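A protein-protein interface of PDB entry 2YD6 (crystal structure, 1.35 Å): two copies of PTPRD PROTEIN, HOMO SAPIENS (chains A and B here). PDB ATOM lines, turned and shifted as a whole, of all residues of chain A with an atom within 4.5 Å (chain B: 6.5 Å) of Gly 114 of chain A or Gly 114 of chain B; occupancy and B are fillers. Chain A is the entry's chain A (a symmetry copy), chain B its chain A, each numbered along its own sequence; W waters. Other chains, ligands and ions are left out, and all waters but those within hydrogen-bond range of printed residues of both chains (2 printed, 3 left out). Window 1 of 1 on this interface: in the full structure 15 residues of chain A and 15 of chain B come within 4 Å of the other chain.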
ATOM      1  N   ILE A 111       7.325 -23.138  -3.968  1.00  0.00           N
ATOM      2  CA  ILE A 111       7.376 -24.440  -4.616  1.00  0.00           C
ATOM      3  C   ILE A 111       8.647 -24.391  -5.482  1.00  0.00           C
ATOM      4  O   ILE A 111       8.687 -23.745  -6.541  1.00  0.00           O
ATOM      5  CB  ILE A 111       6.162 -24.802  -5.471  1.00  0.00           C
ATOM      6  CG1 ILE A 111       4.835 -24.647  -4.705  1.00  0.00           C
ATOM      7  CG2 ILE A 111       6.336 -26.216  -6.024  1.00  0.00           C
ATOM      8  CD1 ILE A 111       4.720 -25.462  -3.426  1.00  0.00           C
ATOM      9  N   MET A 113      10.337 -26.972  -6.897  1.00  0.00           N
ATOM     10  CA  MET A 113      10.102 -27.805  -8.070  1.00  0.00           C
ATOM     11  C   MET A 113       8.786 -28.515  -7.827  1.00  0.00           C
ATOM     12  O   MET A 113       8.466 -28.859  -6.677  1.00  0.00           O
ATOM     13  CB  MET A 113      11.143 -28.896  -8.221  1.00  0.00           C
ATOM     14  CG  MET A 113      12.540 -28.432  -8.334  1.00  0.00           C
ATOM     15  SD  MET A 113      13.769 -29.755  -8.359  1.00  0.00           S
ATOM     16  CE  MET A 113      14.046 -30.010  -6.602  1.00  0.00           C
ATOM     17  N   GLY A 114       8.031 -28.745  -8.884  1.00  0.00           N
ATOM     18  CA  GLY A 114       6.703 -29.295  -8.769  1.00  0.00           C
ATOM     19  C   GLY A 114       6.461 -30.542  -9.561  1.00  0.00           C
ATOM     20  O   GLY A 114       7.229 -30.893 -10.471  1.00  0.00           O
ATOM     21  N   PRO A 115       5.323 -31.178  -9.297  1.00  0.00           N
ATOM     22  CA  PRO A 115       4.994 -32.445  -9.941  1.00  0.00           C
ATOM     23  C   PRO A 115       4.801 -32.310 -11.447  1.00  0.00           C
ATOM     24  O   PRO A 115       4.519 -31.223 -11.940  1.00  0.00           O
ATOM     25  CB  PRO A 115       3.741 -32.901  -9.192  1.00  0.00           C
ATOM     26  CG  PRO A 115       3.141 -31.606  -8.703  1.00  0.00           C
ATOM     27  CD  PRO A 115       4.310 -30.780  -8.309  1.00  0.00           C
ATOM     28  N   GLN A 116       5.001 -33.416 -12.156  1.00  0.00           N
ATOM     29  CA  GLN A 116       4.971 -33.451 -13.602  1.00  0.00           C
ATOM     30  C   GLN A 116       4.018 -34.514 -14.115  1.00  0.00           C
ATOM     31  O   GLN A 116       3.760 -35.516 -13.466  1.00  0.00           O
ATOM     32  CB  GLN A 116       6.367 -33.727 -14.147  1.00  0.00           C
ATOM     33  CG  GLN A 116       7.417 -32.702 -13.742  1.00  0.00           C
ATOM     34  CD  GLN A 116       7.217 -31.341 -14.396  1.00  0.00           C
ATOM     35  OE1 GLN A 116       6.893 -30.319 -13.739  1.00  0.00           O
ATOM     36  NE2 GLN A 116       7.429 -31.291 -15.672  1.00  0.00           N
ATOM     37  N   LEU A 129       5.872 -35.883  -7.153  1.00  0.00           N
ATOM     38  CA  LEU A 129       6.902 -35.296  -6.339  1.00  0.00           C
ATOM     39  C   LEU A 129       6.806 -33.775  -6.302  1.00  0.00           C
ATOM     40  O   LEU A 129       6.393 -33.133  -7.267  1.00  0.00           O
ATOM     41  CB  LEU A 129       8.267 -35.698  -6.881  1.00  0.00           C
ATOM     42  CG  LEU A 129       8.676 -37.173  -6.721  1.00  0.00           C
ATOM     43  CD1 LEU A 129       9.929 -37.463  -7.550  1.00  0.00           C
ATOM     44  CD2 LEU A 129       8.881 -37.552  -5.250  1.00  0.00           C
ATOM     45  N   SER A 195       1.674 -25.552  -6.296  1.00  0.00           N
ATOM     46  CA  SER A 195       2.418 -25.915  -7.504  1.00  0.00           C
ATOM     47  C   SER A 195       1.553 -25.759  -8.728  1.00  0.00           C
ATOM     48  O   SER A 195       0.326 -25.726  -8.638  1.00  0.00           O
ATOM     49  CB  SER A 195       2.892 -27.367  -7.452  1.00  0.00           C
ATOM     50  OG  SER A 195       1.861 -28.304  -7.670  1.00  0.00           O
ATOM     51  N   ILE B 111      11.195 -36.417 -16.098  1.00  0.00           N
ATOM     52  CA  ILE B 111      11.277 -35.179 -15.337  1.00  0.00           C
ATOM     53  C   ILE B 111      10.535 -35.483 -14.025  1.00  0.00           C
ATOM     54  O   ILE B 111       9.295 -35.551 -13.980  1.00  0.00           O
ATOM     55  CB  ILE B 111      10.681 -33.946 -16.014  1.00  0.00           C
ATOM     56  CG1 ILE B 111      11.234 -33.728 -17.435  1.00  0.00           C
ATOM     57  CG2 ILE B 111      10.904 -32.722 -15.125  1.00  0.00           C
ATOM     58  CD1 ILE B 111      12.746 -33.585 -17.532  1.00  0.00           C
ATOM     59  N   ASP B 112      11.299 -35.729 -12.973  1.00  0.00           N
ATOM     60  CA  ASP B 112      10.725 -36.114 -11.688  1.00  0.00           C
ATOM     61  C   ASP B 112      10.018 -34.944 -11.035  1.00  0.00           C
ATOM     62  O   ASP B 112       8.952 -35.107 -10.448  1.00  0.00           O
ATOM     63  CB  ASP B 112      11.834 -36.664 -10.795  1.00  0.00           C
ATOM     64  CG  ASP B 112      12.534 -37.865 -11.412  1.00  0.00           C
ATOM     65  OD1 ASP B 112      11.850 -38.719 -11.972  1.00  0.00           O
ATOM     66  OD2 ASP B 112      13.763 -37.928 -11.342  1.00  0.00           O
ATOM     67  N   MET B 113      10.626 -33.760 -11.102  1.00  0.00           N
ATOM     68  CA  MET B 113      10.012 -32.518 -10.647  1.00  0.00           C
ATOM     69  C   MET B 113      10.540 -31.428 -11.557  1.00  0.00           C
ATOM     70  O   MET B 113      11.700 -31.489 -11.996  1.00  0.00           O
ATOM     71  CB  MET B 113      10.449 -32.139  -9.246  1.00  0.00           C
ATOM     72  CG  MET B 113      10.158 -33.136  -8.196  1.00  0.00           C
ATOM     73  SD  MET B 113      10.823 -32.725  -6.568  1.00  0.00           S
ATOM     74  CE  MET B 113      12.483 -33.403  -6.686  1.00  0.00           C
ATOM     75  N   GLY B 114       9.715 -30.438 -11.838  1.00  0.00           N
ATOM     76  CA  GLY B 114      10.051 -29.410 -12.791  1.00  0.00           C
ATOM     77  C   GLY B 114       9.974 -28.009 -12.270  1.00  0.00           C
ATOM     78  O   GLY B 114       9.377 -27.741 -11.215  1.00  0.00           O
ATOM     79  N   PRO B 115      10.487 -27.072 -13.062  1.00  0.00           N
ATOM     80  CA  PRO B 115      10.545 -25.675 -12.647  1.00  0.00           C
ATOM     81  C   PRO B 115       9.165 -25.052 -12.473  1.00  0.00           C
ATOM     82  O   PRO B 115       8.191 -25.535 -13.042  1.00  0.00           O
ATOM     83  CB  PRO B 115      11.388 -25.021 -13.744  1.00  0.00           C
ATOM     84  CG  PRO B 115      11.156 -25.916 -14.937  1.00  0.00           C
ATOM     85  CD  PRO B 115      11.122 -27.288 -14.371  1.00  0.00           C
ATOM     86  N   GLN B 116       9.101 -24.011 -11.649  1.00  0.00           N
ATOM     87  CA  GLN B 116       7.861 -23.366 -11.277  1.00  0.00           C
ATOM     88  C   GLN B 116       7.916 -21.869 -11.525  1.00  0.00           C
ATOM     89  O   GLN B 116       8.968 -21.250 -11.502  1.00  0.00           O
ATOM     90  CB  GLN B 116       7.561 -23.617  -9.805  1.00  0.00           C
ATOM     91  CG  GLN B 116       7.434 -25.086  -9.429  1.00  0.00           C
ATOM     92  CD  GLN B 116       6.188 -25.751  -9.998  1.00  0.00           C
ATOM     93  OE1 GLN B 116       6.245 -26.644 -10.881  1.00  0.00           O
ATOM     94  NE2 GLN B 116       5.060 -25.360  -9.497  1.00  0.00           N
ATOM     95  N   LEU B 129      14.690 -24.657 -11.184  1.00  0.00           N
ATOM     96  CA  LEU B 129      15.135 -25.953 -10.750  1.00  0.00           C
ATOM     97  C   LEU B 129      14.413 -27.081 -11.480  1.00  0.00           C
ATOM     98  O   LEU B 129      13.246 -26.961 -11.852  1.00  0.00           O
ATOM     99  CB  LEU B 129      14.899 -26.096  -9.253  1.00  0.00           C
ATOM    100  CG  LEU B 129      15.779 -25.240  -8.323  1.00  0.00           C
ATOM    101  CD1 LEU B 129      15.235 -25.293  -6.894  1.00  0.00           C
ATOM    102  CD2 LEU B 129      17.250 -25.669  -8.375  1.00  0.00           C
ATOM    103  N   CYS B 130      15.106 -28.212 -11.614  1.00  0.00           N
ATOM    104  CA  CYS B 130      14.601 -29.350 -12.314  1.00  0.00           C
ATOM    105  C   CYS B 130      15.248 -30.600 -11.724  1.00  0.00           C
ATOM    106  O   CYS B 130      16.406 -30.559 -11.388  1.00  0.00           O
ATOM    107  CB  CYS B 130      14.995 -29.223 -13.804  1.00  0.00           C
ATOM    108  SG  CYS B 130      14.224 -30.478 -14.849  1.00  0.00           S
ATOM    109  N   ALA B 131      14.517 -31.705 -11.638  1.00  0.00           N
ATOM    110  CA  ALA B 131      15.061 -33.009 -11.198  1.00  0.00           C
ATOM    111  C   ALA B 131      14.720 -34.012 -12.278  1.00  0.00           C
ATOM    112  O   ALA B 131      13.544 -34.160 -12.647  1.00  0.00           O
ATOM    113  CB  ALA B 131      14.447 -33.410  -9.891  1.00  0.00           C
ATOM    114  N   CYS B 184      12.909 -27.122 -18.759  1.00  0.00           N
ATOM    115  CA  CYS B 184      13.982 -28.041 -18.503  1.00  0.00           C
ATOM    116  C   CYS B 184      13.873 -29.201 -19.482  1.00  0.00           C
ATOM    117  O   CYS B 184      12.758 -29.665 -19.756  1.00  0.00           O
ATOM    118  CB  CYS B 184      13.837 -28.547 -17.057  1.00  0.00           C
ATOM    119  SG  CYS B 184      14.881 -29.966 -16.666  1.00  0.00           S
ATOM    120  N   SER B 195      10.216 -30.810 -19.382  1.00  0.00           N
ATOM    121  CA  SER B 195       9.365 -30.396 -18.263  1.00  0.00           C
ATOM    122  C   SER B 195       8.201 -29.575 -18.756  1.00  0.00           C
ATOM    123  O   SER B 195       8.231 -29.031 -19.860  1.00  0.00           O
ATOM    124  CB  SER B 195      10.140 -29.546 -17.257  1.00  0.00           C
ATOM    125  OG  SER B 195      10.387 -28.230 -17.704  1.00  0.00           O
ATOM    126  N   ALA B 196       7.193 -29.392 -17.919  1.00  0.00           N
ATOM    127  CA  ALA B 196       6.210 -28.359 -18.145  1.00  0.00           C
ATOM    128  C   ALA B 196       6.965 -27.002 -18.111  1.00  0.00           C
ATOM    129  O   ALA B 196       7.983 -26.840 -17.447  1.00  0.00           O
ATOM    130  CB  ALA B 196       5.127 -28.399 -17.057  1.00  0.00           C
ATOM    131  N   ALA B 198       7.694 -23.003 -17.171  1.00  0.00           N
ATOM    132  CA  ALA B 198       7.624 -22.169 -15.984  1.00  0.00           C
ATOM    133  C   ALA B 198       7.976 -20.758 -16.351  1.00  0.00           C
ATOM    134  O   ALA B 198       9.043 -20.528 -16.908  1.00  0.00           O
ATOM    135  CB  ALA B 198       8.584 -22.678 -14.920  1.00  0.00           C
HETATM  136  O   HOH W   1       6.165 -35.520 -10.186  1.00  0.00           O
HETATM  137  O   HOH W   2       4.049 -28.662 -10.867  1.00  0.00           O
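The backbone NH (N) of Asp 112 of chain B sits at hydrogen-bond distance from the backbone carbonyl oxygen (O) of Ala 131 of chain B (2.8 Å). O of Met 113 of chain B is in hydrogen-bond range of N of Ala 131 of chain B. The backbone carbonyl oxygen (O) of Gly 114 of chain B sits close to the side-chain amide oxygen (OE1) of Gln 116 of chain B, 3.3 Å away. The side-chain sulfur of Cys 130 of chain B forms a disulfide with the side-chain sulfur of Cys 184 of chain B, 2.0 Å away. O of Cys 184 of chain B lies within hydrogen-bond range of N of Ser 195 of chain B (2.8 Å). O of Gly 114 of chain A lies close to OE1 of Gln 116 of chain A (3.3 Å).
Water W2 lies within hydrogen-bond range of the backbone carbonyl oxygen of Pro 115 of chain A (2.8 Å) and the side-chain amide oxygen of Gln 116 of chain B (3.0 Å). Water W1 lies within hydrogen-bond range of O of Asp 112 of chain B (2.8 Å), N of Leu 129 of chain A (3.1 Å) and N of Gln 116 of chain A (3.1 Å).
Of the 7 printed residues of chain A, 6 touch a printed residue of chain B. Hydrophobic or aromatic side chains of chain A that line the printed part of chain B: Ile 111, Met 113 and Leu 129. Of the 13 printed residues of chain B, 10 touch a printed residue of chain A. Printed residues of chain B that touch a printed residue of chain A: Ile 111, Asp 112, Met 113, Gly 114, Gln 116, Leu 129, Cys 130, Ala 131, Ser 195 and Ala 196. Hydrophobic or aromatic side chains of chain B that line the printed part of chain A: Ile 111, Met 113, Leu 129 and Ala 196. Along chain B the printed residues that touch a printed residue of chain A span positions 111 to 196. Among the printed residues, 16 pairs touch across the chains. Among the printed residues, no Asp or Glu carboxylate lies within 4 Å of a Lys or Arg side-chain nitrogen of the other chain.
Of chain A, only Met 113 (3.2 Å), Gly 114 (2.9 Å) and Gln 116 (3.4 Å) come within 4 Å of Gly 114 of chain B. Of the printed residues of chain A, Gln 116 of chain B touches Ile 111, Gly 114 and Ser 195. Of the printed residues of chain B, Met 113 of chain A touches Met 113 (3.5 Å), Gly 114 (3.2 Å), Leu 129 (3.4 Å), Cys 130 (3.8 Å) and Ala 131 (3.9 Å). Of the printed residues of chain A, Ile 111 of chain B touches Gln 116 (3.4 Å). Pro 115 of chain A touches none of the printed residues of chain B. Pro 115 of chain B touches none of the printed residues of chain A. The nearest printed residue of chain A that does not touch Gly 114 of chain B is Pro 115 of chain A (5.1 Å).
Ile 111 of chain A touches Gln 116 of chain B, and with the chains exchanged Gln 116 of chain A touches Ile 111 of chain B. Met 113 of chain A touches Gly 114 of chain B, and with the chains exchanged Gly 114 of chain A touches Met 113 of chain B. Met 113 of chain A touches Leu 129 of chain B, and with the chains exchanged Leu 129 of chain A touches Met 113 of chain B. Gly 114 of chain A touches its own counterpart, Gly 114 of chain B. Positions printed for both chains: 111, 113, 114, 115, 116, 129 and 195. Of the 16 pairs that touch across the chains among the printed residues, 12 have their exchanged pair printed and touching as well.
Among the printed residues, pairs that only touch across the chains: Gly 114 of chain A with Met 113 of chain B, Met 113 of chain A with Gly 114 of chain B, Ser 195 of chain A with Gln 116 of chain B, Gln 116 of chain A with Ser 195 of chain B, Gln 116 of chain A with Ile 111 of chain B, Ile 111 of chain A with Gln 116 of chain B, Met 113 of chain A with Leu 129 of chain B, Leu 129 of chain A with Met 113 of chain B, Met 113 of chain A with Met 113 of chain B, Leu 129 of chain A with Asp 112 of chain B, Met 113 of chain A with Cys 130 of chain B and Met 113 of chain A with Ala 131 of chain B.
O of Gly 114 of chain A is in hydrogen-bond range of N of Gly 114 of chain B. The backbone NH (N) of Gly 114 of chain B lies within hydrogen-bond range of the side-chain amide oxygen (OE1) of Gln 116 of chain A, 3.4 Å away. The backbone NH of Gly 114 of chain A sits at hydrogen-bond distance from the side-chain amide oxygen of Gln 116 of chain B, 3.4 Å away. The backbone NH (N) of Ala 196 of chain B lies close to the side-chain amide nitrogen (NE2) of Gln 116 of chain A (3.0 Å).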
